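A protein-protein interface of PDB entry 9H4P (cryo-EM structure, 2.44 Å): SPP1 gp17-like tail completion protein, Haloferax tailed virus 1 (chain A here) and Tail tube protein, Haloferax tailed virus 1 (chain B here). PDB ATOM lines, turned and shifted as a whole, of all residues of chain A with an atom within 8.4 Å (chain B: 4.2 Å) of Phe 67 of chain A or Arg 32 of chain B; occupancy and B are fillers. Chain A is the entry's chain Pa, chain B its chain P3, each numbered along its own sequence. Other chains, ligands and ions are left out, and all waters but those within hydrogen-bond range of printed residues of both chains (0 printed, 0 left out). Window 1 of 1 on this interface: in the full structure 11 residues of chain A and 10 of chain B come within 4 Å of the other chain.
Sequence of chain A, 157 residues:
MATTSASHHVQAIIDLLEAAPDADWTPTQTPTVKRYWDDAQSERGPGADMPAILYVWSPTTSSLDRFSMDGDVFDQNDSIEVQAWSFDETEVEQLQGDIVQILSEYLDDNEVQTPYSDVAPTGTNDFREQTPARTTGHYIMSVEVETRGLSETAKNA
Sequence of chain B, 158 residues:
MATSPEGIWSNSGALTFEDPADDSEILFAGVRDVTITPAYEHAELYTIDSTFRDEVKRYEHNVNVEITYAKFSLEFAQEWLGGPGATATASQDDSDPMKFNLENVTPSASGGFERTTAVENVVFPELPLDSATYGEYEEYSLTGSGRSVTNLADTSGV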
ATOM      1  N   LEU A  64     -18.804 -11.139  11.686  1.00  0.00           N
ATOM      2  CA  LEU A  64     -17.883 -11.273  12.808  1.00  0.00           C
ATOM      3  C   LEU A  64     -18.531 -10.662  14.053  1.00  0.00           C
ATOM      4  O   LEU A  64     -18.376  -9.469  14.307  1.00  0.00           O
ATOM      5  CB  LEU A  64     -16.549 -10.581  12.481  1.00  0.00           C
ATOM      6  CG  LEU A  64     -15.673 -11.224  11.400  1.00  0.00           C
ATOM      7  CD1 LEU A  64     -14.525 -10.305  11.001  1.00  0.00           C
ATOM      8  CD2 LEU A  64     -15.124 -12.570  11.858  1.00  0.00           C
ATOM      9  N   ASP A  65     -19.270 -11.482  14.815  1.00  0.00           N
ATOM     10  CA  ASP A  65     -19.919 -11.033  16.040  1.00  0.00           C
ATOM     11  C   ASP A  65     -18.956 -11.171  17.220  1.00  0.00           C
ATOM     12  O   ASP A  65     -18.163 -12.111  17.257  1.00  0.00           O
ATOM     13  CB  ASP A  65     -21.229 -11.789  16.293  1.00  0.00           C
ATOM     14  CG  ASP A  65     -22.343 -11.483  15.305  1.00  0.00           C
ATOM     15  OD1 ASP A  65     -22.306 -10.407  14.681  1.00  0.00           O
ATOM     16  OD2 ASP A  65     -23.245 -12.325  15.175  1.00  0.00           O
ATOM     17  N   ARG A  66     -19.042 -10.236  18.180  1.00  0.00           N
ATOM     18  CA  ARG A  66     -18.341 -10.335  19.456  1.00  0.00           C
ATOM     19  C   ARG A  66     -18.858 -11.553  20.225  1.00  0.00           C
ATOM     20  O   ARG A  66     -20.070 -11.722  20.359  1.00  0.00           O
ATOM     21  CB  ARG A  66     -18.557  -9.061  20.285  1.00  0.00           C
ATOM     22  CG  ARG A  66     -17.863  -7.817  19.742  1.00  0.00           C
ATOM     23  CD  ARG A  66     -16.339  -7.841  19.772  1.00  0.00           C
ATOM     24  NE  ARG A  66     -15.865  -8.105  21.127  1.00  0.00           N
ATOM     25  CZ  ARG A  66     -15.293  -7.219  21.938  1.00  0.00           C
ATOM     26  NH1 ARG A  66     -14.934  -7.585  23.156  1.00  0.00           N
ATOM     27  NH2 ARG A  66     -15.078  -5.976  21.540  1.00  0.00           N
ATOM     28  N   PHE A  67     -17.940 -12.384  20.738  1.00  0.00           N
ATOM     29  CA  PHE A  67     -18.312 -13.564  21.509  1.00  0.00           C
ATOM     30  C   PHE A  67     -18.519 -13.237  22.994  1.00  0.00           C
ATOM     31  O   PHE A  67     -19.360 -13.864  23.645  1.00  0.00           O
ATOM     32  CB  PHE A  67     -17.299 -14.695  21.288  1.00  0.00           C
ATOM     33  CG  PHE A  67     -17.665 -16.014  21.923  1.00  0.00           C
ATOM     34  CD1 PHE A  67     -18.739 -16.759  21.447  1.00  0.00           C
ATOM     35  CD2 PHE A  67     -16.931 -16.523  22.989  1.00  0.00           C
ATOM     36  CE1 PHE A  67     -19.078 -17.976  22.026  1.00  0.00           C
ATOM     37  CE2 PHE A  67     -17.268 -17.741  23.567  1.00  0.00           C
ATOM     38  CZ  PHE A  67     -18.341 -18.465  23.086  1.00  0.00           C
ATOM     39  N   SER A  68     -17.745 -12.265  23.519  1.00  0.00           N
ATOM     40  CA  SER A  68     -17.740 -11.894  24.934  1.00  0.00           C
ATOM     41  C   SER A  68     -17.042 -10.548  25.161  1.00  0.00           C
ATOM     42  O   SER A  68     -16.480  -9.977  24.227  1.00  0.00           O
ATOM     43  CB  SER A  68     -17.121 -12.998  25.781  1.00  0.00           C
ATOM     44  OG  SER A  68     -15.777 -13.273  25.402  1.00  0.00           O
ATOM     45  N   MET A  69     -17.078 -10.061  26.415  1.00  0.00           N
ATOM     46  CA  MET A  69     -16.353  -8.884  26.873  1.00  0.00           C
ATOM     47  C   MET A  69     -14.831  -9.070  26.778  1.00  0.00           C
ATOM     48  O   MET A  69     -14.112  -8.071  26.768  1.00  0.00           O
ATOM     49  CB  MET A  69     -16.757  -8.517  28.310  1.00  0.00           C
ATOM     50  CG  MET A  69     -18.056  -7.710  28.400  1.00  0.00           C
ATOM     51  SD  MET A  69     -18.837  -7.592  30.039  1.00  0.00           S
ATOM     52  CE  MET A  69     -17.456  -7.053  31.046  1.00  0.00           C
ATOM     53  N   ASP A  70     -14.333 -10.318  26.694  1.00  0.00           N
ATOM     54  CA  ASP A  70     -12.897 -10.577  26.629  1.00  0.00           C
ATOM     55  C   ASP A  70     -12.287 -10.059  25.322  1.00  0.00           C
ATOM     56  O   ASP A  70     -11.151  -9.587  25.328  1.00  0.00           O
ATOM     57  CB  ASP A  70     -12.556 -12.063  26.798  1.00  0.00           C
ATOM     58  CG  ASP A  70     -12.814 -12.644  28.178  1.00  0.00           C
ATOM     59  OD1 ASP A  70     -13.229 -11.888  29.078  1.00  0.00           O
ATOM     60  OD2 ASP A  70     -12.596 -13.857  28.339  1.00  0.00           O
ATOM     61  N   GLY A  71     -13.024 -10.196  24.208  1.00  0.00           N
ATOM     62  CA  GLY A  71     -12.557  -9.811  22.880  1.00  0.00           C
ATOM     63  C   GLY A  71     -11.498 -10.751  22.300  1.00  0.00           C
ATOM     64  O   GLY A  71     -10.858 -10.414  21.305  1.00  0.00           O
ATOM     65  N   ASP A  72     -11.346 -11.930  22.922  1.00  0.00           N
ATOM     66  CA  ASP A  72     -10.358 -12.954  22.606  1.00  0.00           C
ATOM     67  C   ASP A  72     -10.704 -13.701  21.311  1.00  0.00           C
ATOM     68  O   ASP A  72      -9.818 -14.307  20.704  1.00  0.00           O
ATOM     69  CB  ASP A  72     -10.263 -13.914  23.798  1.00  0.00           C
ATOM     70  CG  ASP A  72      -9.222 -15.010  23.675  1.00  0.00           C
ATOM     71  OD1 ASP A  72      -8.055 -14.687  23.396  1.00  0.00           O
ATOM     72  OD2 ASP A  72      -9.589 -16.179  23.866  1.00  0.00           O
ATOM     73  N   VAL A  73     -11.988 -13.652  20.898  1.00  0.00           N
ATOM     74  CA  VAL A  73     -12.558 -14.460  19.820  1.00  0.00           C
ATOM     75  C   VAL A  73     -13.729 -13.712  19.168  1.00  0.00           C
ATOM     76  O   VAL A  73     -14.434 -12.957  19.840  1.00  0.00           O
ATOM     77  CB  VAL A  73     -12.981 -15.852  20.356  1.00  0.00           C
ATOM     78  CG1 VAL A  73     -14.259 -16.415  19.744  1.00  0.00           C
ATOM     79  CG2 VAL A  73     -11.858 -16.881  20.288  1.00  0.00           C
ATOM     80  N   PHE A  74     -13.939 -13.954  17.861  1.00  0.00           N
ATOM     81  CA  PHE A  74     -15.172 -13.625  17.155  1.00  0.00           C
ATOM     82  C   PHE A  74     -15.995 -14.896  16.919  1.00  0.00           C
ATOM     83  O   PHE A  74     -15.439 -15.938  16.574  1.00  0.00           O
ATOM     84  CB  PHE A  74     -14.865 -13.017  15.781  1.00  0.00           C
ATOM     85  CG  PHE A  74     -14.128 -11.699  15.760  1.00  0.00           C
ATOM     86  CD1 PHE A  74     -14.714 -10.543  16.264  1.00  0.00           C
ATOM     87  CD2 PHE A  74     -12.870 -11.602  15.179  1.00  0.00           C
ATOM     88  CE1 PHE A  74     -14.043  -9.328  16.219  1.00  0.00           C
ATOM     89  CE2 PHE A  74     -12.201 -10.386  15.129  1.00  0.00           C
ATOM     90  CZ  PHE A  74     -12.788  -9.253  15.653  1.00  0.00           C
ATOM     91  N   ASP A  75     -17.320 -14.800  17.104  1.00  0.00           N
ATOM     92  CA  ASP A  75     -18.266 -15.774  16.576  1.00  0.00           C
ATOM     93  C   ASP A  75     -18.449 -15.473  15.087  1.00  0.00           C
ATOM     94  O   ASP A  75     -19.151 -14.528  14.732  1.00  0.00           O
ATOM     95  CB  ASP A  75     -19.574 -15.726  17.378  1.00  0.00           C
ATOM     96  CG  ASP A  75     -20.693 -16.647  16.916  1.00  0.00           C
ATOM     97  OD1 ASP A  75     -20.475 -17.441  15.981  1.00  0.00           O
ATOM     98  OD2 ASP A  75     -21.780 -16.565  17.514  1.00  0.00           O
ATOM     99  N   GLN A  76     -17.787 -16.265  14.231  1.00  0.00           N
ATOM    100  CA  GLN A  76     -17.746 -16.000  12.799  1.00  0.00           C
ATOM    101  C   GLN A  76     -18.742 -16.904  12.072  1.00  0.00           C
ATOM    102  O   GLN A  76     -18.699 -18.124  12.231  1.00  0.00           O
ATOM    103  CB  GLN A  76     -16.321 -16.171  12.263  1.00  0.00           C
ATOM    104  CG  GLN A  76     -16.219 -15.939  10.760  1.00  0.00           C
ATOM    105  CD  GLN A  76     -14.814 -15.918  10.211  1.00  0.00           C
ATOM    106  OE1 GLN A  76     -13.832 -15.827  10.944  1.00  0.00           O
ATOM    107  NE2 GLN A  76     -14.708 -15.995   8.896  1.00  0.00           N
ATOM    108  N   ARG A 148     -19.746 -22.039  10.519  1.00  0.00           N
ATOM    109  CA  ARG A 148     -19.642 -21.266  11.746  1.00  0.00           C
ATOM    110  C   ARG A 148     -18.488 -21.776  12.605  1.00  0.00           C
ATOM    111  O   ARG A 148     -18.244 -22.980  12.672  1.00  0.00           O
ATOM    112  CB  ARG A 148     -20.975 -21.290  12.501  1.00  0.00           C
ATOM    113  CG  ARG A 148     -21.087 -20.237  13.594  1.00  0.00           C
ATOM    114  CD  ARG A 148     -22.478 -20.261  14.186  1.00  0.00           C
ATOM    115  NE  ARG A 148     -22.656 -19.299  15.264  1.00  0.00           N
ATOM    116  CZ  ARG A 148     -23.776 -19.148  15.963  1.00  0.00           C
ATOM    117  NH1 ARG A 148     -23.838 -18.245  16.926  1.00  0.00           N
ATOM    118  NH2 ARG A 148     -24.833 -19.898  15.709  1.00  0.00           N
ATOM    119  N   GLY A 149     -17.794 -20.842  13.262  1.00  0.00           N
ATOM    120  CA  GLY A 149     -16.709 -21.186  14.165  1.00  0.00           C
ATOM    121  C   GLY A 149     -16.256 -19.993  14.997  1.00  0.00           C
ATOM    122  O   GLY A 149     -16.492 -18.842  14.625  1.00  0.00           O
ATOM    123  N   LEU A 150     -15.604 -20.294  16.127  1.00  0.00           N
ATOM    124  CA  LEU A 150     -14.863 -19.290  16.873  1.00  0.00           C
ATOM    125  C   LEU A 150     -13.571 -18.976  16.114  1.00  0.00           C
ATOM    126  O   LEU A 150     -12.883 -19.891  15.661  1.00  0.00           O
ATOM    127  CB  LEU A 150     -14.603 -19.795  18.299  1.00  0.00           C
ATOM    128  CG  LEU A 150     -15.835 -20.135  19.144  1.00  0.00           C
ATOM    129  CD1 LEU A 150     -15.433 -20.424  20.583  1.00  0.00           C
ATOM    130  CD2 LEU A 150     -16.888 -19.030  19.113  1.00  0.00           C
ATOM    131  N   SER A 151     -13.269 -17.675  15.974  1.00  0.00           N
ATOM    132  CA  SER A 151     -12.170 -17.162  15.165  1.00  0.00           C
ATOM    133  C   SER A 151     -11.312 -16.234  16.030  1.00  0.00           C
ATOM    134  O   SER A 151     -11.863 -15.424  16.770  1.00  0.00           O
ATOM    135  CB  SER A 151     -12.732 -16.436  13.959  1.00  0.00           C
ATOM    136  OG  SER A 151     -11.719 -16.101  13.022  1.00  0.00           O
ATOM    137  N   THR A 153      -8.337 -13.484  17.639  1.00  0.00           N
ATOM    138  CA  THR A 153      -8.042 -12.053  17.583  1.00  0.00           C
ATOM    139  C   THR A 153      -6.627 -11.766  18.096  1.00  0.00           C
ATOM    140  O   THR A 153      -6.051 -12.574  18.823  1.00  0.00           O
ATOM    141  CB  THR A 153      -9.049 -11.209  18.387  1.00  0.00           C
ATOM    142  OG1 THR A 153      -8.806 -11.376  19.784  1.00  0.00           O
ATOM    143  CG2 THR A 153     -10.501 -11.511  18.091  1.00  0.00           C
ATOM    144  N   GLY B  30     -14.862 -15.076  29.470  1.00  0.00           N
ATOM    145  CA  GLY B  30     -15.926 -14.977  28.479  1.00  0.00           C
ATOM    146  C   GLY B  30     -17.243 -14.418  29.016  1.00  0.00           C
ATOM    147  O   GLY B  30     -18.306 -14.871  28.591  1.00  0.00           O
ATOM    148  N   VAL B  31     -17.171 -13.410  29.901  1.00  0.00           N
ATOM    149  CA  VAL B  31     -18.368 -12.785  30.459  1.00  0.00           C
ATOM    150  C   VAL B  31     -19.100 -11.976  29.381  1.00  0.00           C
ATOM    151  O   VAL B  31     -18.481 -11.451  28.451  1.00  0.00           O
ATOM    152  CB  VAL B  31     -18.096 -11.961  31.740  1.00  0.00           C
ATOM    153  CG1 VAL B  31     -17.535 -12.822  32.866  1.00  0.00           C
ATOM    154  CG2 VAL B  31     -17.213 -10.738  31.502  1.00  0.00           C
ATOM    155  N   ARG B  32     -20.431 -11.895  29.541  1.00  0.00           N
ATOM    156  CA  ARG B  32     -21.333 -11.182  28.644  1.00  0.00           C
ATOM    157  C   ARG B  32     -22.116 -10.118  29.415  1.00  0.00           C
ATOM    158  O   ARG B  32     -22.277  -9.000  28.924  1.00  0.00           O
ATOM    159  CB  ARG B  32     -22.253 -12.164  27.911  1.00  0.00           C
ATOM    160  CG  ARG B  32     -21.543 -12.928  26.804  1.00  0.00           C
ATOM    161  CD  ARG B  32     -22.468 -13.888  26.089  1.00  0.00           C
ATOM    162  NE  ARG B  32     -21.793 -14.490  24.947  1.00  0.00           N
ATOM    163  CZ  ARG B  32     -22.308 -15.406  24.128  1.00  0.00           C
ATOM    164  NH1 ARG B  32     -21.575 -15.869  23.131  1.00  0.00           N
ATOM    165  NH2 ARG B  32     -23.534 -15.869  24.305  1.00  0.00           N
ATOM    166  N   ASP B  33     -22.606 -10.479  30.613  1.00  0.00           N
ATOM    167  CA  ASP B  33     -23.220  -9.541  31.544  1.00  0.00           C
ATOM    168  C   ASP B  33     -22.532  -9.674  32.906  1.00  0.00           C
ATOM    169  O   ASP B  33     -22.184 -10.786  33.307  1.00  0.00           O
ATOM    170  CB  ASP B  33     -24.718  -9.817  31.746  1.00  0.00           C
ATOM    171  CG  ASP B  33     -25.524 -10.229  30.524  1.00  0.00           C
ATOM    172  OD1 ASP B  33     -25.207  -9.765  29.415  1.00  0.00           O
ATOM    173  OD2 ASP B  33     -26.486 -10.992  30.701  1.00  0.00           O
ATOM    174  N   THR B  68     -23.470 -13.379  33.516  1.00  0.00           N
ATOM    175  CA  THR B  68     -23.716 -14.232  32.358  1.00  0.00           C
ATOM    176  C   THR B  68     -22.394 -14.426  31.611  1.00  0.00           C
ATOM    177  O   THR B  68     -21.702 -13.443  31.338  1.00  0.00           O
ATOM    178  CB  THR B  68     -24.731 -13.600  31.392  1.00  0.00           C
ATOM    179  OG1 THR B  68     -25.900 -13.190  32.103  1.00  0.00           O
ATOM    180  CG2 THR B  68     -25.132 -14.505  30.247  1.00  0.00           C
ATOM    181  N   ALA B  70     -19.886 -17.224  28.732  1.00  0.00           N
ATOM    182  CA  ALA B  70     -20.002 -18.095  27.565  1.00  0.00           C
ATOM    183  C   ALA B  70     -18.788 -19.005  27.327  1.00  0.00           C
ATOM    184  O   ALA B  70     -18.805 -19.796  26.379  1.00  0.00           O
ATOM    185  CB  ALA B  70     -20.329 -17.272  26.339  1.00  0.00           C
ATOM    186  N   LYS B  71     -17.742 -18.897  28.164  1.00  0.00           N
ATOM    187  CA  LYS B  71     -16.630 -19.842  28.157  1.00  0.00           C
ATOM    188  C   LYS B  71     -16.719 -20.697  29.421  1.00  0.00           C
ATOM    189  O   LYS B  71     -16.688 -20.157  30.527  1.00  0.00           O
ATOM    190  CB  LYS B  71     -15.281 -19.111  28.113  1.00  0.00           C
ATOM    191  CG  LYS B  71     -14.906 -18.450  26.793  1.00  0.00           C
ATOM    192  CD  LYS B  71     -13.512 -17.862  26.829  1.00  0.00           C
ATOM    193  CE  LYS B  71     -13.003 -17.429  25.473  1.00  0.00           C
ATOM    194  NZ  LYS B  71     -11.559 -17.106  25.530  1.00  0.00           N
ATOM    195  N   TYR B 137     -23.657 -21.597  20.766  1.00  0.00           N
ATOM    196  CA  TYR B 137     -22.663 -21.845  21.803  1.00  0.00           C
ATOM    197  C   TYR B 137     -23.336 -21.731  23.170  1.00  0.00           C
ATOM    198  O   TYR B 137     -24.249 -20.924  23.336  1.00  0.00           O
ATOM    199  CB  TYR B 137     -21.477 -20.883  21.666  1.00  0.00           C
ATOM    200  CG  TYR B 137     -20.694 -21.088  20.394  1.00  0.00           C
ATOM    201  CD1 TYR B 137     -19.667 -22.019  20.335  1.00  0.00           C
ATOM    202  CD2 TYR B 137     -21.008 -20.382  19.238  1.00  0.00           C
ATOM    203  CE1 TYR B 137     -18.960 -22.232  19.161  1.00  0.00           C
ATOM    204  CE2 TYR B 137     -20.310 -20.582  18.057  1.00  0.00           C
ATOM    205  CZ  TYR B 137     -19.285 -21.513  18.021  1.00  0.00           C
ATOM    206  OH  TYR B 137     -18.592 -21.704  16.860  1.00  0.00           O
ATOM    207  N   GLU B 139     -24.292 -20.852  26.985  1.00  0.00           N
ATOM    208  CA  GLU B 139     -24.268 -19.642  27.801  1.00  0.00           C
ATOM    209  C   GLU B 139     -24.761 -19.976  29.212  1.00  0.00           C
ATOM    210  O   GLU B 139     -25.729 -20.718  29.371  1.00  0.00           O
ATOM    211  CB  GLU B 139     -25.112 -18.548  27.137  1.00  0.00           C
ATOM    212  CG  GLU B 139     -25.040 -17.197  27.822  1.00  0.00           C
ATOM    213  CD  GLU B 139     -25.857 -16.130  27.124  1.00  0.00           C
ATOM    214  OE1 GLU B 139     -27.076 -16.075  27.354  1.00  0.00           O
ATOM    215  OE2 GLU B 139     -25.275 -15.372  26.338  1.00  0.00           O
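Hydrophobic or aromatic side chains of chain B within 4 Å of the printed part of chain A: Val 31, Ala 70 and Tyr 137.
Printed residues of chain A that touch a printed residue of chain B: Phe 67, Ser 68, Met 69, Asp 70, Asp 72, Asp 75, Arg 148, Gly 149 and Leu 150.
Among the printed residues, Asp or Glu carboxylates within 4 Å of a Lys or Arg side-chain nitrogen of the other chain: Asp 72 of chain A with Lys 71 of chain B (2.7 Å).
Ala 70 of chain B touches Phe 67 of chain A.
Phe 67 of chain A touches Tyr 137 of chain B.
OG of Ser 68 of chain A touches CA of Gly 30 of chain B (3.5 Å).
Ser 68 of chain A touches Val 31 of chain B (CB to O, 3.4 Å).
Arg 32 of chain B touches Met 69 of chain A.
OD1 of Asp 75 of chain A touches CE2 of Tyr 137 of chain B, at 3.8 Å.
Tyr 137 of chain B touches Arg 148 of chain A.
Gly 149 of chain A touches Tyr 137 of chain B.
The backbone NH of Gly 30 of chain B lies within hydrogen-bond range of the side-chain carboxylate of Asp 70 of chain A, 2.8 Å away.
NZ of Lys 71 of chain B is in salt-bridge range of OD2 of Asp 72 of chain A (2.7 Å).
The backbone NH (N) of Met 69 of chain A sits at hydrogen-bond distance from the backbone carbonyl oxygen (O) of Val 31 of chain B (2.8 Å).
The guanidinium group (NE) of Arg 32 of chain B is in hydrogen-bond range of the backbone carbonyl oxygen (O) of Phe 67 of chain A (2.8 Å).
OH of Tyr 137 of chain B sits at hydrogen-bond distance from N of Leu 150 of chain A, at 3.4 Å.
The backbone carbonyl oxygen (O) of Asp 72 of chain A is in hydrogen-bond range of the side-chain hydroxyl (OG1) of Thr 153 of chain A (3.2 Å).
The guanidinium group of Arg 32 of chain B is in salt-bridge range of the side-chain carboxylate of Glu 139 of chain B, 2.7 Å away.
The backbone NH (N) of Asp 75 of chain A sits at hydrogen-bond distance from the backbone carbonyl oxygen (O) of Asp 65 of chain A (2.8 Å).
OD2 of Asp 75 of chain A lies within salt-bridge range of NH1 of Arg 148 of chain A.
The backbone carbonyl oxygen (O) of Gly 30 of chain B lies within hydrogen-bond range of the backbone NH (N) of Ala 70 of chain B (2.8 Å).
N of Arg 32 of chain B sits at hydrogen-bond distance from O of Thr 68 of chain B (2.7 Å).
Of the printed residues of chain A, Gly 30 of chain B touches Ser 68 (3.5 Å) and Asp 70 (2.8 Å).
Printed residues of chain B within 4 Å of Asp 72 of chain A: Lys 71.
Thr 68 of chain B touches none of the printed residues of chain A.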
